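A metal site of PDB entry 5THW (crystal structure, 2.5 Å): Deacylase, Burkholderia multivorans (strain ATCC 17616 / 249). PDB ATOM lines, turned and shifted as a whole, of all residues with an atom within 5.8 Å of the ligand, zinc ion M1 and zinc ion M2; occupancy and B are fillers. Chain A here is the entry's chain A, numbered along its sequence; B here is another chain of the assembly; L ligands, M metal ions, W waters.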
ATOM      1  N   SER A 103     -29.169  12.875 -30.812  1.00  0.00           N
ATOM      2  CA  SER A 103     -28.870  12.682 -29.402  1.00  0.00           C
ATOM      3  C   SER A 103     -28.129  13.915 -28.920  1.00  0.00           C
ATOM      4  O   SER A 103     -28.447  15.030 -29.347  1.00  0.00           O
ATOM      5  CB  SER A 103     -28.059  11.392 -29.206  1.00  0.00           C
ATOM      6  OG  SER A 103     -28.279  10.832 -27.928  1.00  0.00           O
ATOM      7  N   HIS A 104     -27.135  13.743 -28.061  1.00  0.00           N
ATOM      8  CA  HIS A 104     -26.385  14.865 -27.538  1.00  0.00           C
ATOM      9  C   HIS A 104     -24.903  14.647 -27.782  1.00  0.00           C
ATOM     10  O   HIS A 104     -24.418  13.523 -27.837  1.00  0.00           O
ATOM     11  CB  HIS A 104     -26.627  15.060 -26.048  1.00  0.00           C
ATOM     12  CG  HIS A 104     -26.358  13.835 -25.227  1.00  0.00           C
ATOM     13  ND1 HIS A 104     -25.170  13.647 -24.549  1.00  0.00           N
ATOM     14  CD2 HIS A 104     -27.100  12.739 -24.994  1.00  0.00           C
ATOM     15  CE1 HIS A 104     -25.210  12.486 -23.921  1.00  0.00           C
ATOM     16  NE2 HIS A 104     -26.376  11.911 -24.169  1.00  0.00           N
ATOM     17  N   GLN A 108     -20.360  13.823 -19.626  1.00  0.00           N
ATOM     18  CA  GLN A 108     -20.027  13.959 -18.226  1.00  0.00           C
ATOM     19  C   GLN A 108     -18.545  14.325 -18.056  1.00  0.00           C
ATOM     20  O   GLN A 108     -17.762  14.204 -19.002  1.00  0.00           O
ATOM     21  CB  GLN A 108     -20.342  12.656 -17.482  1.00  0.00           C
ATOM     22  CG  GLN A 108     -21.823  12.367 -17.416  1.00  0.00           C
ATOM     23  CD  GLN A 108     -22.506  13.182 -16.334  1.00  0.00           C
ATOM     24  OE1 GLN A 108     -21.870  13.651 -15.395  1.00  0.00           O
ATOM     25  NE2 GLN A 108     -23.817  13.367 -16.468  1.00  0.00           N
ATOM     26  N   ASP A 115     -21.617   7.554 -25.135  1.00  0.00           N
ATOM     27  CA  ASP A 115     -22.811   8.169 -24.570  1.00  0.00           C
ATOM     28  C   ASP A 115     -23.185   9.423 -25.368  1.00  0.00           C
ATOM     29  O   ASP A 115     -22.395  10.362 -25.459  1.00  0.00           O
ATOM     30  CB  ASP A 115     -22.538   8.496 -23.105  1.00  0.00           C
ATOM     31  CG  ASP A 115     -23.761   9.013 -22.358  1.00  0.00           C
ATOM     32  OD1 ASP A 115     -24.858   9.124 -22.943  1.00  0.00           O
ATOM     33  OD2 ASP A 115     -23.600   9.332 -21.155  1.00  0.00           O
ATOM     34  N   GLY A 116     -24.386   9.417 -25.953  1.00  0.00           N
ATOM     35  CA  GLY A 116     -24.865  10.556 -26.715  1.00  0.00           C
ATOM     36  C   GLY A 116     -24.341  10.701 -28.128  1.00  0.00           C
ATOM     37  O   GLY A 116     -25.109  10.755 -29.091  1.00  0.00           O
ATOM     38  N   GLU A 149     -27.835  17.891 -22.550  1.00  0.00           N
ATOM     39  CA  GLU A 149     -28.691  16.751 -22.205  1.00  0.00           C
ATOM     40  C   GLU A 149     -28.281  16.130 -20.886  1.00  0.00           C
ATOM     41  O   GLU A 149     -29.135  15.682 -20.120  1.00  0.00           O
ATOM     42  CB  GLU A 149     -28.686  15.715 -23.327  1.00  0.00           C
ATOM     43  CG  GLU A 149     -29.634  14.556 -23.103  1.00  0.00           C
ATOM     44  CD  GLU A 149     -29.026  13.443 -22.268  1.00  0.00           C
ATOM     45  OE1 GLU A 149     -27.777  13.424 -22.120  1.00  0.00           O
ATOM     46  OE2 GLU A 149     -29.781  12.589 -21.770  1.00  0.00           O
ATOM     47  N   GLU A 150     -26.976  16.106 -20.594  1.00  0.00           N
ATOM     48  CA  GLU A 150     -26.465  15.410 -19.409  1.00  0.00           C
ATOM     49  C   GLU A 150     -27.007  16.017 -18.123  1.00  0.00           C
ATOM     50  O   GLU A 150     -27.210  15.294 -17.137  1.00  0.00           O
ATOM     51  CB  GLU A 150     -24.938  15.441 -19.396  1.00  0.00           C
ATOM     52  CG  GLU A 150     -24.274  14.497 -20.385  1.00  0.00           C
ATOM     53  CD  GLU A 150     -24.408  13.036 -19.995  1.00  0.00           C
ATOM     54  OE1 GLU A 150     -24.946  12.753 -18.901  1.00  0.00           O
ATOM     55  OE2 GLU A 150     -23.987  12.166 -20.790  1.00  0.00           O
ATOM     56  N   ALA A 157     -31.270  17.572 -16.407  1.00  0.00           N
ATOM     57  CA  ALA A 157     -31.012  16.944 -17.689  1.00  0.00           C
ATOM     58  C   ALA A 157     -32.123  17.245 -18.700  1.00  0.00           C
ATOM     59  O   ALA A 157     -33.222  17.683 -18.354  1.00  0.00           O
ATOM     60  CB  ALA A 157     -30.865  15.432 -17.514  1.00  0.00           C
ATOM     61  N   MET A 158     -31.793  17.060 -19.982  1.00  0.00           N
ATOM     62  CA  MET A 158     -32.761  17.091 -21.086  1.00  0.00           C
ATOM     63  C   MET A 158     -33.530  18.406 -21.152  1.00  0.00           C
ATOM     64  O   MET A 158     -34.679  18.422 -21.609  1.00  0.00           O
ATOM     65  CB  MET A 158     -33.751  15.928 -20.980  1.00  0.00           C
ATOM     66  CG  MET A 158     -33.128  14.556 -21.050  1.00  0.00           C
ATOM     67  SD  MET A 158     -33.880  13.400 -19.891  1.00  0.00           S
ATOM     68  CE  MET A 158     -35.582  13.385 -20.421  1.00  0.00           C
ATOM     69  N   GLU A 209     -34.242   7.584 -31.442  1.00  0.00           N
ATOM     70  CA  GLU A 209     -32.936   7.861 -30.839  1.00  0.00           C
ATOM     71  C   GLU A 209     -32.158   6.570 -30.638  1.00  0.00           C
ATOM     72  O   GLU A 209     -32.660   5.631 -30.008  1.00  0.00           O
ATOM     73  CB  GLU A 209     -33.084   8.622 -29.517  1.00  0.00           C
ATOM     74  CG  GLU A 209     -31.750   8.976 -28.888  1.00  0.00           C
ATOM     75  CD  GLU A 209     -31.864  10.054 -27.828  1.00  0.00           C
ATOM     76  OE1 GLU A 209     -30.857  10.347 -27.159  1.00  0.00           O
ATOM     77  OE2 GLU A 209     -32.973  10.600 -27.662  1.00  0.00           O
ATOM     78  N   HIS A 211     -28.886   4.704 -28.987  1.00  0.00           N
ATOM     79  CA  HIS A 211     -28.106   4.930 -27.771  1.00  0.00           C
ATOM     80  C   HIS A 211     -27.538   3.612 -27.250  1.00  0.00           C
ATOM     81  O   HIS A 211     -28.101   2.550 -27.520  1.00  0.00           O
ATOM     82  CB  HIS A 211     -28.973   5.592 -26.677  1.00  0.00           C
ATOM     83  CG  HIS A 211     -28.196   6.440 -25.718  1.00  0.00           C
ATOM     84  ND1 HIS A 211     -27.440   5.922 -24.696  1.00  0.00           N
ATOM     85  CD2 HIS A 211     -28.060   7.789 -25.635  1.00  0.00           C
ATOM     86  CE1 HIS A 211     -26.868   6.902 -24.028  1.00  0.00           C
ATOM     87  NE2 HIS A 211     -27.228   8.046 -24.581  1.00  0.00           N
ATOM     88  N   GLN A 214     -26.165   1.637 -21.469  1.00  0.00           N
ATOM     89  CA  GLN A 214     -25.647   2.138 -20.204  1.00  0.00           C
ATOM     90  C   GLN A 214     -25.938   1.182 -19.048  1.00  0.00           C
ATOM     91  O   GLN A 214     -25.834   1.569 -17.874  1.00  0.00           O
ATOM     92  CB  GLN A 214     -26.173   3.551 -19.900  1.00  0.00           C
ATOM     93  CG  GLN A 214     -26.062   4.480 -21.114  1.00  0.00           C
ATOM     94  CD  GLN A 214     -26.583   5.881 -20.857  1.00  0.00           C
ATOM     95  OE1 GLN A 214     -27.784   6.116 -20.859  1.00  0.00           O
ATOM     96  NE2 GLN A 214     -25.669   6.843 -20.664  1.00  0.00           N
ATOM     97  N   GLN A 234     -38.064   9.818 -13.356  1.00  0.00           N
ATOM     98  CA  GLN A 234     -37.018  10.323 -12.482  1.00  0.00           C
ATOM     99  C   GLN A 234     -37.511  11.511 -11.660  1.00  0.00           C
ATOM    100  O   GLN A 234     -38.402  12.256 -12.073  1.00  0.00           O
ATOM    101  CB  GLN A 234     -35.764  10.757 -13.264  1.00  0.00           C
ATOM    102  CG  GLN A 234     -35.249   9.767 -14.289  1.00  0.00           C
ATOM    103  CD  GLN A 234     -33.854  10.120 -14.766  1.00  0.00           C
ATOM    104  OE1 GLN A 234     -33.056  10.658 -14.007  1.00  0.00           O
ATOM    105  NE2 GLN A 234     -33.575   9.855 -16.035  1.00  0.00           N
ATOM    106  N   TRP A 236     -35.365  14.525  -9.329  1.00  0.00           N
ATOM    107  CA  TRP A 236     -34.091  15.078  -8.875  1.00  0.00           C
ATOM    108  C   TRP A 236     -34.328  16.168  -7.837  1.00  0.00           C
ATOM    109  O   TRP A 236     -35.255  16.976  -7.961  1.00  0.00           O
ATOM    110  CB  TRP A 236     -33.273  15.651 -10.041  1.00  0.00           C
ATOM    111  CG  TRP A 236     -32.754  14.645 -11.020  1.00  0.00           C
ATOM    112  CD1 TRP A 236     -33.140  13.336 -11.143  1.00  0.00           C
ATOM    113  CD2 TRP A 236     -31.754  14.865 -12.024  1.00  0.00           C
ATOM    114  NE1 TRP A 236     -32.437  12.736 -12.153  1.00  0.00           N
ATOM    115  CE2 TRP A 236     -31.589  13.643 -12.721  1.00  0.00           C
ATOM    116  CE3 TRP A 236     -30.999  15.977 -12.417  1.00  0.00           C
ATOM    117  CZ2 TRP A 236     -30.680  13.512 -13.777  1.00  0.00           C
ATOM    118  CZ3 TRP A 236     -30.104  15.834 -13.459  1.00  0.00           C
ATOM    119  CH2 TRP A 236     -29.952  14.615 -14.124  1.00  0.00           C
ATOM    120  N   ASP A 307     -30.905  11.750  -6.586  1.00  0.00           N
ATOM    121  CA  ASP A 307     -31.328  11.192  -7.863  1.00  0.00           C
ATOM    122  C   ASP A 307     -32.193   9.968  -7.548  1.00  0.00           C
ATOM    123  O   ASP A 307     -31.698   8.981  -6.984  1.00  0.00           O
ATOM    124  CB  ASP A 307     -30.103  10.811  -8.699  1.00  0.00           C
ATOM    125  CG  ASP A 307     -30.454  10.252 -10.089  1.00  0.00           C
ATOM    126  OD1 ASP A 307     -29.941  10.799 -11.095  1.00  0.00           O
ATOM    127  OD2 ASP A 307     -31.230   9.270 -10.185  1.00  0.00           O
ATOM    128  N   ARG A 309     -34.992   7.165  -9.279  1.00  0.00           N
ATOM    129  CA  ARG A 309     -35.532   6.623 -10.519  1.00  0.00           C
ATOM    130  C   ARG A 309     -36.329   5.364 -10.230  1.00  0.00           C
ATOM    131  O   ARG A 309     -35.968   4.589  -9.345  1.00  0.00           O
ATOM    132  CB  ARG A 309     -34.436   6.309 -11.540  1.00  0.00           C
ATOM    133  CG  ARG A 309     -33.522   7.477 -11.830  1.00  0.00           C
ATOM    134  CD  ARG A 309     -32.457   7.170 -12.853  1.00  0.00           C
ATOM    135  NE  ARG A 309     -31.423   8.192 -12.812  1.00  0.00           N
ATOM    136  CZ  ARG A 309     -30.739   8.614 -13.863  1.00  0.00           C
ATOM    137  NH1 ARG A 309     -30.980   8.105 -15.071  1.00  0.00           N
ATOM    138  NH2 ARG A 309     -29.804   9.548 -13.716  1.00  0.00           N
ATOM    139  N   TYR A 346     -40.270  13.752 -14.258  1.00  0.00           N
ATOM    140  CA  TYR A 346     -41.032  13.322 -15.417  1.00  0.00           C
ATOM    141  C   TYR A 346     -41.509  11.891 -15.208  1.00  0.00           C
ATOM    142  O   TYR A 346     -40.760  11.050 -14.712  1.00  0.00           O
ATOM    143  CB  TYR A 346     -40.253  13.465 -16.739  1.00  0.00           C
ATOM    144  CG  TYR A 346     -39.082  12.530 -16.944  1.00  0.00           C
ATOM    145  CD1 TYR A 346     -37.791  12.938 -16.626  1.00  0.00           C
ATOM    146  CD2 TYR A 346     -39.255  11.281 -17.527  1.00  0.00           C
ATOM    147  CE1 TYR A 346     -36.720  12.111 -16.836  1.00  0.00           C
ATOM    148  CE2 TYR A 346     -38.180  10.445 -17.747  1.00  0.00           C
ATOM    149  CZ  TYR A 346     -36.918  10.870 -17.398  1.00  0.00           C
ATOM    150  OH  TYR A 346     -35.833  10.053 -17.609  1.00  0.00           O
ATOM    151  N   GLY A 376     -32.977   2.768 -18.610  1.00  0.00           N
ATOM    152  CA  GLY A 376     -32.648   3.194 -17.265  1.00  0.00           C
ATOM    153  C   GLY A 376     -32.287   4.655 -17.136  1.00  0.00           C
ATOM    154  O   GLY A 376     -32.332   5.203 -16.029  1.00  0.00           O
ATOM    155  N   ALA A 377     -31.942   5.306 -18.240  1.00  0.00           N
ATOM    156  CA  ALA A 377     -31.561   6.705 -18.237  1.00  0.00           C
ATOM    157  C   ALA A 377     -32.586   7.519 -19.001  1.00  0.00           C
ATOM    158  O   ALA A 377     -33.408   6.976 -19.758  1.00  0.00           O
ATOM    159  CB  ALA A 377     -30.168   6.922 -18.859  1.00  0.00           C
ATOM    160  N   GLY A 378     -32.536   8.828 -18.796  1.00  0.00           N
ATOM    161  CA  GLY A 378     -33.384   9.730 -19.526  1.00  0.00           C
ATOM    162  C   GLY A 378     -32.686  10.116 -20.821  1.00  0.00           C
ATOM    163  O   GLY A 378     -31.467  10.226 -20.882  1.00  0.00           O
ATOM    164  N   HIS A 379     -33.485  10.306 -21.868  1.00  0.00           N
ATOM    165  CA  HIS A 379     -32.944  10.705 -23.143  1.00  0.00           C
ATOM    166  C   HIS A 379     -33.861  11.772 -23.711  1.00  0.00           C
ATOM    167  O   HIS A 379     -35.000  11.928 -23.279  1.00  0.00           O
ATOM    168  CB  HIS A 379     -32.820   9.505 -24.092  1.00  0.00           C
ATOM    169  CG  HIS A 379     -32.081   8.343 -23.500  1.00  0.00           C
ATOM    170  ND1 HIS A 379     -30.711   8.329 -23.326  1.00  0.00           N
ATOM    171  CD2 HIS A 379     -32.528   7.152 -23.033  1.00  0.00           C
ATOM    172  CE1 HIS A 379     -30.351   7.186 -22.772  1.00  0.00           C
ATOM    173  NE2 HIS A 379     -31.437   6.446 -22.593  1.00  0.00           N
ATOM    174  N   SER A 402     -21.448   2.976 -17.949  1.00  0.00           N
ATOM    175  CA  SER A 402     -21.492   4.273 -18.608  1.00  0.00           C
ATOM    176  C   SER A 402     -21.244   5.337 -17.542  1.00  0.00           C
ATOM    177  O   SER A 402     -21.275   5.061 -16.338  1.00  0.00           O
ATOM    178  CB  SER A 402     -22.817   4.528 -19.324  1.00  0.00           C
ATOM    179  OG  SER A 402     -22.789   5.735 -20.079  1.00  0.00           O
ATOM    180  N   HIS A 403     -20.990   6.566 -18.000  1.00  0.00           N
ATOM    181  CA  HIS A 403     -20.515   7.647 -17.127  1.00  0.00           C
ATOM    182  C   HIS A 403     -19.218   7.258 -16.427  1.00  0.00           C
ATOM    183  O   HIS A 403     -18.944   7.676 -15.295  1.00  0.00           O
ATOM    184  CB  HIS A 403     -21.580   8.097 -16.119  1.00  0.00           C
ATOM    185  CG  HIS A 403     -22.699   8.873 -16.745  1.00  0.00           C
ATOM    186  ND1 HIS A 403     -23.772   9.343 -16.031  1.00  0.00           N
ATOM    187  CD2 HIS A 403     -22.894   9.268 -18.028  1.00  0.00           C
ATOM    188  CE1 HIS A 403     -24.586   9.999 -16.840  1.00  0.00           C
ATOM    189  NE2 HIS A 403     -24.076   9.966 -18.054  1.00  0.00           N
ATOM    190  N   HIS B 247     -22.882   5.282 -13.983  1.00  0.00           N
ATOM    191  CA  HIS B 247     -24.119   6.004 -14.229  1.00  0.00           C
ATOM    192  C   HIS B 247     -25.074   5.842 -13.051  1.00  0.00           C
ATOM    193  O   HIS B 247     -25.252   4.734 -12.529  1.00  0.00           O
ATOM    194  CB  HIS B 247     -24.787   5.493 -15.500  1.00  0.00           C
ATOM    195  CG  HIS B 247     -25.733   6.472 -16.126  1.00  0.00           C
ATOM    196  ND1 HIS B 247     -26.834   6.985 -15.465  1.00  0.00           N
ATOM    197  CD2 HIS B 247     -25.742   7.042 -17.358  1.00  0.00           C
ATOM    198  CE1 HIS B 247     -27.476   7.825 -16.248  1.00  0.00           C
ATOM    199  NE2 HIS B 247     -26.827   7.880 -17.407  1.00  0.00           N
ATOM    200  N   ASN B 296     -25.550  13.046 -11.443  1.00  0.00           N
ATOM    201  CA  ASN B 296     -25.973  11.765 -11.993  1.00  0.00           C
ATOM    202  C   ASN B 296     -24.799  10.831 -12.278  1.00  0.00           C
ATOM    203  O   ASN B 296     -24.847  10.001 -13.195  1.00  0.00           O
ATOM    204  CB  ASN B 296     -26.857  11.970 -13.228  1.00  0.00           C
ATOM    205  CG  ASN B 296     -26.218  12.852 -14.293  1.00  0.00           C
ATOM    206  OD1 ASN B 296     -25.245  13.576 -14.042  1.00  0.00           O
ATOM    207  ND2 ASN B 296     -26.792  12.842 -15.483  1.00  0.00           N
HETATM  208  O1  LIG L   1     -26.852   9.344 -19.584  1.00  0.00           O
HETATM  209  C1  LIG L   1     -27.533  10.133 -20.211  1.00  0.00           C
HETATM  210  N1  LIG L   1     -27.121  10.629 -21.365  1.00  0.00           N
HETATM  211  N2  LIG L   1     -28.713  10.544 -19.741  1.00  0.00           N
HETATM  212  C2  LIG L   1     -28.804  11.739 -18.923  1.00  0.00           C
HETATM  213  C3  LIG L   1     -30.101  11.783 -18.130  1.00  0.00           C
HETATM  214  C4  LIG L   1     -30.008  10.715 -17.073  1.00  0.00           C
HETATM  215  O2  LIG L   1     -30.731   9.689 -17.193  1.00  0.00           O
HETATM  216  O3  LIG L   1     -29.223  10.887 -16.110  1.00  0.00           O
HETATM  217 ZN    ZN M   1     -24.882  10.397 -19.992  1.00  0.00          ZN
HETATM  218 ZN    ZN M   2     -27.124   9.964 -23.242  1.00  0.00          ZN
HETATM  219  O   HOH W   1     -29.314  10.549 -23.701  1.00  0.00           O
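Gln 214 touches zinc ion M1.
Four residues have an atom within 4 Å of zinc ion M1: Asp 115, Glu 150, Gln 214 and His 403.
The nearest printed residue that does not touch zinc ion M1 is His 247 of chain B (4.1 Å).
Gly 116 touches zinc ion M2 (N to ZN, 3.9 Å).
Glu 149 touches zinc ion M2.
ND1 of His 379 touches zinc ion M2, 3.9 Å away.
Within 4 Å of zinc ion M2: His 104, Asp 115, Gly 116, Glu 149, His 211 and His 379.
Zinc ion M2 is bound by N1 of the ligand (2.0 Å), NE2 of His 104 (2.3 Å), water W1 (2.3 Å), NE2 of His 211 (2.3 Å) and OD1 of Asp 115 (2.4 Å).
Zinc ion M2 has five donor atoms within binding distance.
The side-chain amide nitrogen of Gln 214 sits close to the side-chain carboxylate of Asp 115 (3.3 Å).
The backbone carbonyl oxygen (O) of Glu 150 sits at hydrogen-bond distance from the side-chain amide nitrogen (ND2) of Asn 296 of chain B.
The side-chain carboxylate (OE1) of Glu 150 lies close to the side-chain amide nitrogen (NE2) of Gln 108, 2.8 Å away.
A ring nitrogen (ND1) of His 403 sits at hydrogen-bond distance from the backbone carbonyl oxygen of Asn 296 of chain B, at 3.1 Å.
The backbone NH (N) of His 247 of chain B sits at hydrogen-bond distance from the backbone carbonyl oxygen (O) of Ser 402 (2.9 Å).
OE1 of Gln 234 lies within hydrogen-bond range of NE1 of Trp 236 (2.9 Å).
The side-chain amide nitrogen (NE2) of Gln 234 lies within hydrogen-bond range of the side-chain hydroxyl (OH) of Tyr 346 (2.8 Å).
The side-chain carboxylate (OD1) of Asp 307 sits at hydrogen-bond distance from the indole nitrogen (NE1) of Trp 236 (3.3 Å).
N of Gly 378 lies within hydrogen-bond range of O2 of the ligand, 2.6 Å away.
A nitrogen (N2) of the ligand sits at hydrogen-bond distance from the backbone carbonyl oxygen (O) of Gly 378.
NE2 of His 247 of chain B sits close to O1 of the ligand, at 2.6 Å.
NH1 of Arg 309 is in salt-bridge range of O2 of the ligand (2.7 Å).
The side-chain carboxylate (OE2) of Glu 149 sits at hydrogen-bond distance from a nitrogen (N2) of the ligand.
NE2 of Gln 214 sits close to O1 of the ligand.
O2 of the ligand sits at hydrogen-bond distance from NE2 of Gln 234 (3.1 Å).
An oxygen (O3) of the ligand lies within hydrogen-bond range of the side-chain amide nitrogen (ND2) of Asn 296 of chain B, at 3.2 Å.
Water W1 lies within hydrogen-bond range of a ring nitrogen (ND1) of His 379 and the side-chain carboxylate of Glu 149.
Merely in contact with the ligand: Ala 377 (3.3 Å), Ala 157 (3.8 Å) and Trp 236 (3.8 Å).
Hydrophobic or aromatic side chains within 4 Å of the ligand: His 104, Ala 157, Trp 236, Ala 377, His 403 and His 247 of chain B.
14 residues have an atom within 4 Å of the ligand: His 104, Asp 115, Glu 149, Glu 150, Ala 157, Gln 214, Gln 234, Trp 236, Arg 309, Ala 377, Gly 378, His 403, His 247 of chain B and Asn 296 of chain B.
The nearest printed residue that does not touch the ligand is His 211 (4.1 Å).
OD2 of Asp 115 binds zinc ion M1 (2.0 Å).
Zinc ion M1 is bound by OE2 of Glu 150.
NE2 of His 403 is bound to zinc ion M1.
Zinc ion M1 is bound by O1 of the ligand (2.3 Å).
OE1 of Glu 150 is bound to zinc ion M1 (2.6 Å).
Zinc ion M1 has five donor atoms within binding distance.
Slightly farther from zinc ion M1 lies a nitrogen (N1) of the ligand (2.6 Å).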
